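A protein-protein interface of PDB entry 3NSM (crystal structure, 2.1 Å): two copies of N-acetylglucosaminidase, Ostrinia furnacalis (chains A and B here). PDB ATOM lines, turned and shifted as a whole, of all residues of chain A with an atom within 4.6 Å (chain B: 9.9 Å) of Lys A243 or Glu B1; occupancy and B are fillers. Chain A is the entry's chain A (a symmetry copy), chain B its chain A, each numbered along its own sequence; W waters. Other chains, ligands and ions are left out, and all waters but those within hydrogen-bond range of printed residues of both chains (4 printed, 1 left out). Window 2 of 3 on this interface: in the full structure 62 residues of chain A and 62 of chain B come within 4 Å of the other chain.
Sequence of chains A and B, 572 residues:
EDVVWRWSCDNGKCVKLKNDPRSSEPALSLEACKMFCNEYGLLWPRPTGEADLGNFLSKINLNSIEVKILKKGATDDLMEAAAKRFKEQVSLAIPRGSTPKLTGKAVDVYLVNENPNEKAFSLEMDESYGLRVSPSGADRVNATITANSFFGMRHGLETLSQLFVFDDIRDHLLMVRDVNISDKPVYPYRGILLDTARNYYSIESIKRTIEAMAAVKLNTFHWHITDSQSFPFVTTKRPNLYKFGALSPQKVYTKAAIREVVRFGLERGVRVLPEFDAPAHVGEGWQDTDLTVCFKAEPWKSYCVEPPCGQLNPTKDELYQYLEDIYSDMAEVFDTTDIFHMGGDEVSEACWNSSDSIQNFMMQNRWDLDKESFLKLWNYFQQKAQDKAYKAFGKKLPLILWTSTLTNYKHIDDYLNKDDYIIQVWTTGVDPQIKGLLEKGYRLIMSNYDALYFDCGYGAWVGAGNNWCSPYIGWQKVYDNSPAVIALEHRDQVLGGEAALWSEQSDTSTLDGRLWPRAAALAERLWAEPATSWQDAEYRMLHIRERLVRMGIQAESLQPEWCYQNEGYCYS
No position is printed for both chains.
Of the 8 pairs that touch across the chains among the printed residues, none has its exchanged pair printed and touching as well.
O of Val B4 sits at hydrogen-bond distance from N of Asn B19 (3.3 Å).
The side-chain hydroxyl of Tyr A242 sits at hydrogen-bond distance from the side-chain amino group of Lys A243 (3.0 Å).
Water W2 lies within hydrogen-bond range of O of Glu B1 and NE2 of Gln A250.
Water W3 lies within hydrogen-bond range of the backbone NH (N) of Glu B1 and the side-chain amide nitrogen (NE2) of Gln A250.
Water W4 lies within hydrogen-bond range of O of Phe A244 (2.9 Å), NZ of Lys B16 (3.0 Å) and O of Gly A245 (3.2 Å).
Water W1 lies within hydrogen-bond range of the backbone carbonyl oxygen of Lys A243 (2.9 Å), the indole nitrogen of Trp B5 (3.1 Å) and the backbone carbonyl oxygen of Phe A244 (3.3 Å).
Tyr A242 touches just one residue of chain B: Glu B1.
Of the printed residues of chain B, Lys A243 touches Glu B1 (3.98 Å) and Val B4 (3.3 Å).
Of chain B, only Glu B1 (3.3 Å), Asp B2 (3.7 Å) and Val B3 (3.6 Å) come within 4 Å of Pro A249.
Of the printed residues of chain A, Glu B1 touches Tyr A242 (3.7 Å), Lys A243 (3.98 Å) and Pro A249 (3.3 Å).
Printed residues of chain A within 4 Å of Asp B2: Pro A249 (3.7 Å).
Of the printed residues of chain A, Lys B18 touches Phe A244.
Gln B565 touches none of the printed residues of chain A.
The nearest printed residue of chain A that does not touch Glu B1 is Gln A250 (4.4 Å).
The nearest printed residue of chain A that does not touch Val B3 is Gln A250 (6.1 Å).
Printed residues of chain B that touch a printed residue of chain A: Glu B1, Asp B2, Val B3, Val B4, Trp B5 and Lys B18.
Along chain B the printed residues that touch a printed residue of chain A span positions 1 to 18.
Of the 9 printed residues of chain A, 4 touch a printed residue of chain B.
Among the printed residues, no Asp or Glu carboxylate lies within 4 Å of a Lys or Arg side-chain nitrogen of the other chain.
The backbone carbonyl oxygen of Phe A244 is in hydrogen-bond range of the indole nitrogen of Trp B5 (3.0 Å).
Tyr A242 touches Glu B1.
Lys A243 touches Glu B1.
Val B4 touches Lys A243.
NZ of Lys B18 touches CE1 of Phe A244 (3.1 Å).
Pro A249 touches Glu B1.
Pro A249 touches Asp B2 (CG to C, 3.7 Å).
Pro A249 touches Val B3.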
ATOM      1  N   PRO A 239     -19.515  21.630  -6.145  1.00  0.00           N
ATOM      2  CA  PRO A 239     -18.316  22.250  -5.561  1.00  0.00           C
ATOM      3  C   PRO A 239     -17.135  22.391  -6.517  1.00  0.00           C
ATOM      4  O   PRO A 239     -16.323  23.294  -6.345  1.00  0.00           O
ATOM      5  CB  PRO A 239     -17.956  21.313  -4.400  1.00  0.00           C
ATOM      6  CG  PRO A 239     -18.579  19.996  -4.767  1.00  0.00           C
ATOM      7  CD  PRO A 239     -19.854  20.360  -5.475  1.00  0.00           C
ATOM      8  N   ASN A 240     -17.040  21.521  -7.515  1.00  0.00           N
ATOM      9  CA  ASN A 240     -15.987  21.645  -8.518  1.00  0.00           C
ATOM     10  C   ASN A 240     -16.007  22.944  -9.328  1.00  0.00           C
ATOM     11  O   ASN A 240     -14.971  23.360  -9.850  1.00  0.00           O
ATOM     12  CB  ASN A 240     -15.984  20.438  -9.458  1.00  0.00           C
ATOM     13  CG  ASN A 240     -15.316  19.218  -8.840  1.00  0.00           C
ATOM     14  OD1 ASN A 240     -14.846  19.256  -7.700  1.00  0.00           O
ATOM     15  ND2 ASN A 240     -15.270  18.124  -9.598  1.00  0.00           N
ATOM     16  N   LEU A 241     -17.177  23.576  -9.451  1.00  0.00           N
ATOM     17  CA  LEU A 241     -17.265  24.846 -10.175  1.00  0.00           C
ATOM     18  C   LEU A 241     -16.392  25.912  -9.518  1.00  0.00           C
ATOM     19  O   LEU A 241     -15.622  26.576 -10.197  1.00  0.00           O
ATOM     20  CB  LEU A 241     -18.720  25.331 -10.316  1.00  0.00           C
ATOM     21  CG  LEU A 241     -19.669  24.431 -11.115  1.00  0.00           C
ATOM     22  CD1 LEU A 241     -21.113  24.884 -10.933  1.00  0.00           C
ATOM     23  CD2 LEU A 241     -19.290  24.385 -12.586  1.00  0.00           C
ATOM     24  N   TYR A 242     -16.495  26.057  -8.201  1.00  0.00           N
ATOM     25  CA  TYR A 242     -15.671  27.028  -7.493  1.00  0.00           C
ATOM     26  C   TYR A 242     -14.276  26.507  -7.141  1.00  0.00           C
ATOM     27  O   TYR A 242     -13.332  27.289  -7.047  1.00  0.00           O
ATOM     28  CB  TYR A 242     -16.387  27.572  -6.255  1.00  0.00           C
ATOM     29  CG  TYR A 242     -16.373  26.666  -5.051  1.00  0.00           C
ATOM     30  CD1 TYR A 242     -15.287  26.660  -4.173  1.00  0.00           C
ATOM     31  CD2 TYR A 242     -17.461  25.842  -4.761  1.00  0.00           C
ATOM     32  CE1 TYR A 242     -15.272  25.837  -3.052  1.00  0.00           C
ATOM     33  CE2 TYR A 242     -17.458  25.018  -3.642  1.00  0.00           C
ATOM     34  CZ  TYR A 242     -16.357  25.020  -2.793  1.00  0.00           C
ATOM     35  OH  TYR A 242     -16.336  24.202  -1.685  1.00  0.00           O
ATOM     36  N   LYS A 243     -14.139  25.198  -6.947  1.00  0.00           N
ATOM     37  CA  LYS A 243     -12.817  24.620  -6.703  1.00  0.00           C
ATOM     38  C   LYS A 243     -11.938  24.761  -7.940  1.00  0.00           C
ATOM     39  O   LYS A 243     -10.776  25.147  -7.828  1.00  0.00           O
ATOM     40  CB  LYS A 243     -12.915  23.167  -6.245  1.00  0.00           C
ATOM     41  CG  LYS A 243     -13.331  23.011  -4.775  1.00  0.00           C
ATOM     42  CD  LYS A 243     -13.925  21.633  -4.510  1.00  0.00           C
ATOM     43  CE  LYS A 243     -13.692  21.161  -3.074  1.00  0.00           C
ATOM     44  NZ  LYS A 243     -14.327  22.042  -2.043  1.00  0.00           N
ATOM     45  N   PHE A 244     -12.495  24.487  -9.115  1.00  0.00           N
ATOM     46  CA  PHE A 244     -11.754  24.668 -10.362  1.00  0.00           C
ATOM     47  C   PHE A 244     -11.772  26.116 -10.854  1.00  0.00           C
ATOM     48  O   PHE A 244     -10.828  26.554 -11.513  1.00  0.00           O
ATOM     49  CB  PHE A 244     -12.272  23.761 -11.486  1.00  0.00           C
ATOM     50  CG  PHE A 244     -12.152  22.278 -11.211  1.00  0.00           C
ATOM     51  CD1 PHE A 244     -12.849  21.369 -12.008  1.00  0.00           C
ATOM     52  CD2 PHE A 244     -11.359  21.789 -10.170  1.00  0.00           C
ATOM     53  CE1 PHE A 244     -12.757  19.994 -11.781  1.00  0.00           C
ATOM     54  CE2 PHE A 244     -11.267  20.415  -9.920  1.00  0.00           C
ATOM     55  CZ  PHE A 244     -11.961  19.516 -10.728  1.00  0.00           C
ATOM     56  N   GLY A 245     -12.844  26.846 -10.534  1.00  0.00           N
ATOM     57  CA  GLY A 245     -13.093  28.157 -11.126  1.00  0.00           C
ATOM     58  C   GLY A 245     -12.524  29.369 -10.421  1.00  0.00           C
ATOM     59  O   GLY A 245     -12.213  30.364 -11.068  1.00  0.00           O
ATOM     60  N   PRO A 249      -7.888  29.637  -3.747  1.00  0.00           N
ATOM     61  CA  PRO A 249      -8.818  29.124  -2.734  1.00  0.00           C
ATOM     62  C   PRO A 249      -9.396  30.186  -1.803  1.00  0.00           C
ATOM     63  O   PRO A 249     -10.473  29.983  -1.263  1.00  0.00           O
ATOM     64  CB  PRO A 249      -7.947  28.148  -1.926  1.00  0.00           C
ATOM     65  CG  PRO A 249      -6.844  27.773  -2.855  1.00  0.00           C
ATOM     66  CD  PRO A 249      -6.552  29.023  -3.609  1.00  0.00           C
ATOM     67  N   GLN A 250      -8.692  31.296  -1.601  1.00  0.00           N
ATOM     68  CA  GLN A 250      -9.169  32.347  -0.692  1.00  0.00           C
ATOM     69  C   GLN A 250     -10.094  33.341  -1.399  1.00  0.00           C
ATOM     70  O   GLN A 250     -10.879  34.038  -0.751  1.00  0.00           O
ATOM     71  CB  GLN A 250      -8.003  33.104  -0.046  1.00  0.00           C
ATOM     72  CG  GLN A 250      -7.233  32.311   1.006  1.00  0.00           C
ATOM     73  CD  GLN A 250      -6.361  31.213   0.410  1.00  0.00           C
ATOM     74  OE1 GLN A 250      -5.676  31.415  -0.606  1.00  0.00           O
ATOM     75  NE2 GLN A 250      -6.382  30.038   1.040  1.00  0.00           N
ATOM     76  N   GLU B   1      -9.444  26.172   1.188  1.00  0.00           N
ATOM     77  CA  GLU B   1      -8.920  24.816   0.832  1.00  0.00           C
ATOM     78  C   GLU B   1      -7.621  24.860  -0.002  1.00  0.00           C
ATOM     79  O   GLU B   1      -6.823  25.795   0.137  1.00  0.00           O
ATOM     80  CB  GLU B   1     -10.016  23.951   0.182  1.00  0.00           C
ATOM     81  CG  GLU B   1     -11.184  24.718  -0.468  1.00  0.00           C
ATOM     82  CD  GLU B   1     -10.981  25.008  -1.956  1.00  0.00           C
ATOM     83  OE1 GLU B   1     -11.591  25.985  -2.464  1.00  0.00           O
ATOM     84  OE2 GLU B   1     -10.223  24.262  -2.622  1.00  0.00           O
ATOM     85  N   ASP B   2      -7.413  23.848  -0.847  1.00  0.00           N
ATOM     86  CA  ASP B   2      -6.149  23.654  -1.574  1.00  0.00           C
ATOM     87  C   ASP B   2      -6.159  24.178  -3.004  1.00  0.00           C
ATOM     88  O   ASP B   2      -7.166  24.064  -3.711  1.00  0.00           O
ATOM     89  CB  ASP B   2      -5.800  22.163  -1.634  1.00  0.00           C
ATOM     90  CG  ASP B   2      -5.471  21.572  -0.270  1.00  0.00           C
ATOM     91  OD1 ASP B   2      -5.870  20.407  -0.028  1.00  0.00           O
ATOM     92  OD2 ASP B   2      -4.810  22.254   0.552  1.00  0.00           O
ATOM     93  N   VAL B   3      -5.021  24.725  -3.431  1.00  0.00           N
ATOM     94  CA  VAL B   3      -4.791  25.077  -4.832  1.00  0.00           C
ATOM     95  C   VAL B   3      -4.875  23.806  -5.684  1.00  0.00           C
ATOM     96  O   VAL B   3      -4.239  22.792  -5.364  1.00  0.00           O
ATOM     97  CB  VAL B   3      -3.413  25.760  -5.019  1.00  0.00           C
ATOM     98  CG1 VAL B   3      -3.157  26.094  -6.476  1.00  0.00           C
ATOM     99  CG2 VAL B   3      -3.318  27.019  -4.169  1.00  0.00           C
ATOM    100  N   VAL B   4      -5.668  23.862  -6.755  1.00  0.00           N
ATOM    101  CA  VAL B   4      -5.947  22.683  -7.581  1.00  0.00           C
ATOM    102  C   VAL B   4      -5.228  22.692  -8.929  1.00  0.00           C
ATOM    103  O   VAL B   4      -5.268  21.701  -9.658  1.00  0.00           O
ATOM    104  CB  VAL B   4      -7.474  22.473  -7.813  1.00  0.00           C
ATOM    105  CG1 VAL B   4      -8.240  22.489  -6.488  1.00  0.00           C
ATOM    106  CG2 VAL B   4      -8.030  23.508  -8.765  1.00  0.00           C
ATOM    107  N   TRP B   5      -4.574  23.805  -9.254  1.00  0.00           N
ATOM    108  CA  TRP B   5      -3.878  23.939 -10.531  1.00  0.00           C
ATOM    109  C   TRP B   5      -2.357  23.902 -10.373  1.00  0.00           C
ATOM    110  O   TRP B   5      -1.837  24.069  -9.273  1.00  0.00           O
ATOM    111  CB  TRP B   5      -4.290  25.238 -11.230  1.00  0.00           C
ATOM    112  CG  TRP B   5      -5.759  25.311 -11.541  1.00  0.00           C
ATOM    113  CD1 TRP B   5      -6.715  25.975 -10.831  1.00  0.00           C
ATOM    114  CD2 TRP B   5      -6.436  24.685 -12.640  1.00  0.00           C
ATOM    115  NE1 TRP B   5      -7.951  25.810 -11.423  1.00  0.00           N
ATOM    116  CE2 TRP B   5      -7.807  25.025 -12.536  1.00  0.00           C
ATOM    117  CE3 TRP B   5      -6.017  23.878 -13.709  1.00  0.00           C
ATOM    118  CZ2 TRP B   5      -8.765  24.573 -13.454  1.00  0.00           C
ATOM    119  CZ3 TRP B   5      -6.972  23.431 -14.629  1.00  0.00           C
ATOM    120  CH2 TRP B   5      -8.333  23.783 -14.489  1.00  0.00           C
ATOM    121  N   TRP B   7       1.303  25.004 -13.059  1.00  0.00           N
ATOM    122  CA  TRP B   7       1.684  25.710 -14.281  1.00  0.00           C
ATOM    123  C   TRP B   7       2.932  25.111 -14.926  1.00  0.00           C
ATOM    124  O   TRP B   7       3.825  24.640 -14.231  1.00  0.00           O
ATOM    125  CB  TRP B   7       1.875  27.210 -14.006  1.00  0.00           C
ATOM    126  CG  TRP B   7       0.571  27.934 -13.769  1.00  0.00           C
ATOM    127  CD1 TRP B   7      -0.118  28.701 -14.667  1.00  0.00           C
ATOM    128  CD2 TRP B   7      -0.210  27.920 -12.570  1.00  0.00           C
ATOM    129  NE1 TRP B   7      -1.270  29.182 -14.094  1.00  0.00           N
ATOM    130  CE2 TRP B   7      -1.352  28.719 -12.806  1.00  0.00           C
ATOM    131  CE3 TRP B   7      -0.051  27.322 -11.313  1.00  0.00           C
ATOM    132  CZ2 TRP B   7      -2.338  28.925 -11.835  1.00  0.00           C
ATOM    133  CZ3 TRP B   7      -1.034  27.534 -10.340  1.00  0.00           C
ATOM    134  CH2 TRP B   7      -2.159  28.333 -10.610  1.00  0.00           C
ATOM    135  N   LYS B  16      -1.641  27.016 -17.535  1.00  0.00           N
ATOM    136  CA  LYS B  16      -2.359  26.435 -16.409  1.00  0.00           C
ATOM    137  C   LYS B  16      -2.866  25.047 -16.779  1.00  0.00           C
ATOM    138  O   LYS B  16      -3.533  24.862 -17.804  1.00  0.00           O
ATOM    139  CB  LYS B  16      -3.513  27.336 -15.944  1.00  0.00           C
ATOM    140  CG  LYS B  16      -4.059  26.965 -14.559  1.00  0.00           C
ATOM    141  CD  LYS B  16      -5.175  27.904 -14.084  1.00  0.00           C
ATOM    142  CE  LYS B  16      -6.524  27.578 -14.731  1.00  0.00           C
ATOM    143  NZ  LYS B  16      -7.660  28.268 -14.036  1.00  0.00           N
ATOM    144  N   LYS B  18      -4.263  21.114 -14.924  1.00  0.00           N
ATOM    145  CA  LYS B  18      -4.752  20.472 -13.724  1.00  0.00           C
ATOM    146  C   LYS B  18      -3.585  19.765 -13.043  1.00  0.00           C
ATOM    147  O   LYS B  18      -2.723  19.188 -13.717  1.00  0.00           O
ATOM    148  CB  LYS B  18      -5.855  19.481 -14.057  1.00  0.00           C
ATOM    149  CG  LYS B  18      -6.889  19.371 -12.973  1.00  0.00           C
ATOM    150  CD  LYS B  18      -8.251  19.154 -13.598  1.00  0.00           C
ATOM    151  CE  LYS B  18      -9.286  20.055 -12.956  1.00  0.00           C
ATOM    152  NZ  LYS B  18     -10.468  20.208 -13.852  1.00  0.00           N
ATOM    153  N   ASN B  19      -3.548  19.851 -11.715  1.00  0.00           N
ATOM    154  CA  ASN B  19      -2.540  19.153 -10.925  1.00  0.00           C
ATOM    155  C   ASN B  19      -3.042  17.745 -10.630  1.00  0.00           C
ATOM    156  O   ASN B  19      -3.526  17.464  -9.527  1.00  0.00           O
ATOM    157  CB  ASN B  19      -2.231  19.922  -9.628  1.00  0.00           C
ATOM    158  CG  ASN B  19      -1.020  19.366  -8.872  1.00  0.00           C
ATOM    159  OD1 ASN B  19      -0.764  19.749  -7.722  1.00  0.00           O
ATOM    160  ND2 ASN B  19      -0.275  18.472  -9.509  1.00  0.00           N
ATOM    161  N   GLY B  97      -2.548  36.414   4.785  1.00  0.00           N
ATOM    162  CA  GLY B  97      -3.354  35.313   5.305  1.00  0.00           C
ATOM    163  C   GLY B  97      -2.748  33.939   5.063  1.00  0.00           C
ATOM    164  O   GLY B  97      -3.206  32.948   5.642  1.00  0.00           O
ATOM    165  N   SER B  98      -1.733  33.877   4.198  1.00  0.00           N
ATOM    166  CA  SER B  98      -0.946  32.657   3.987  1.00  0.00           C
ATOM    167  C   SER B  98       0.252  32.630   4.930  1.00  0.00           C
ATOM    168  O   SER B  98       0.823  33.675   5.247  1.00  0.00           O
ATOM    169  CB  SER B  98      -0.470  32.546   2.534  1.00  0.00           C
ATOM    170  OG  SER B  98      -1.473  32.003   1.695  1.00  0.00           O
ATOM    171  N   ASP B 168       2.383  28.424  -3.116  1.00  0.00           N
ATOM    172  CA  ASP B 168       1.104  28.296  -2.413  1.00  0.00           C
ATOM    173  C   ASP B 168       0.485  26.903  -2.541  1.00  0.00           C
ATOM    174  O   ASP B 168      -0.503  26.595  -1.864  1.00  0.00           O
ATOM    175  CB  ASP B 168       0.110  29.386  -2.846  1.00  0.00           C
ATOM    176  CG  ASP B 168      -0.063  29.456  -4.352  1.00  0.00           C
ATOM    177  OD1 ASP B 168       0.795  28.928  -5.093  1.00  0.00           O
ATOM    178  OD2 ASP B 168      -1.065  30.061  -4.797  1.00  0.00           O
ATOM    179  N   ILE B 169       1.068  26.068  -3.403  1.00  0.00           N
ATOM    180  CA  ILE B 169       0.690  24.658  -3.478  1.00  0.00           C
ATOM    181  C   ILE B 169       1.208  23.950  -2.225  1.00  0.00           C
ATOM    182  O   ILE B 169       0.465  23.225  -1.562  1.00  0.00           O
ATOM    183  CB  ILE B 169       1.237  23.956  -4.756  1.00  0.00           C
ATOM    184  CG1 ILE B 169       0.694  24.625  -6.025  1.00  0.00           C
ATOM    185  CG2 ILE B 169       0.871  22.482  -4.754  1.00  0.00           C
ATOM    186  CD1 ILE B 169       1.281  24.088  -7.321  1.00  0.00           C
ATOM    187  N   ARG B 170       2.473  24.205  -1.890  1.00  0.00           N
ATOM    188  CA  ARG B 170       3.141  23.521  -0.787  1.00  0.00           C
ATOM    189  C   ARG B 170       3.274  24.349   0.497  1.00  0.00           C
ATOM    190  O   ARG B 170       3.633  23.807   1.544  1.00  0.00           O
ATOM    191  CB  ARG B 170       4.510  23.004  -1.254  1.00  0.00           C
ATOM    192  CG  ARG B 170       4.407  21.749  -2.099  1.00  0.00           C
ATOM    193  CD  ARG B 170       5.747  21.262  -2.623  1.00  0.00           C
ATOM    194  NE  ARG B 170       6.049  21.900  -3.894  1.00  0.00           N
ATOM    195  CZ  ARG B 170       5.834  21.366  -5.091  1.00  0.00           C
ATOM    196  NH1 ARG B 170       5.341  20.148  -5.225  1.00  0.00           N
ATOM    197  NH2 ARG B 170       6.132  22.067  -6.170  1.00  0.00           N
ATOM    198  N   ASP B 171       2.960  25.644   0.420  1.00  0.00           N
ATOM    199  CA  ASP B 171       3.221  26.605   1.506  1.00  0.00           C
ATOM    200  C   ASP B 171       4.720  26.704   1.825  1.00  0.00           C
ATOM    201  O   ASP B 171       5.120  26.684   2.986  1.00  0.00           O
ATOM    202  CB  ASP B 171       2.403  26.284   2.771  1.00  0.00           C
ATOM    203  CG  ASP B 171       0.943  26.695   2.653  1.00  0.00           C
ATOM    204  OD1 ASP B 171       0.633  27.631   1.881  1.00  0.00           O
ATOM    205  OD2 ASP B 171       0.098  26.081   3.344  1.00  0.00           O
ATOM    206  N   GLN B 565      -2.762  34.581 -14.771  1.00  0.00           N
ATOM    207  CA  GLN B 565      -2.708  33.135 -14.567  1.00  0.00           C
ATOM    208  C   GLN B 565      -2.670  32.345 -15.868  1.00  0.00           C
ATOM    209  O   GLN B 565      -2.419  31.136 -15.853  1.00  0.00           O
ATOM    210  CB  GLN B 565      -3.896  32.667 -13.723  1.00  0.00           C
ATOM    211  CG  GLN B 565      -3.867  33.219 -12.324  1.00  0.00           C
ATOM    212  CD  GLN B 565      -4.872  32.584 -11.390  1.00  0.00           C
ATOM    213  OE1 GLN B 565      -4.998  33.008 -10.241  1.00  0.00           O
ATOM    214  NE2 GLN B 565      -5.593  31.576 -11.865  1.00  0.00           N
HETATM  215  O   HOH W   1      -8.958  27.202  -8.902  1.00  0.00           O
HETATM  216  O   HOH W   2      -4.824  27.539   0.563  1.00  0.00           O
HETATM  217  O   HOH W   3      -8.753  28.668   2.129  1.00  0.00           O
HETATM  218  O   HOH W   4      -9.442  29.029 -11.792  1.00  0.00           O
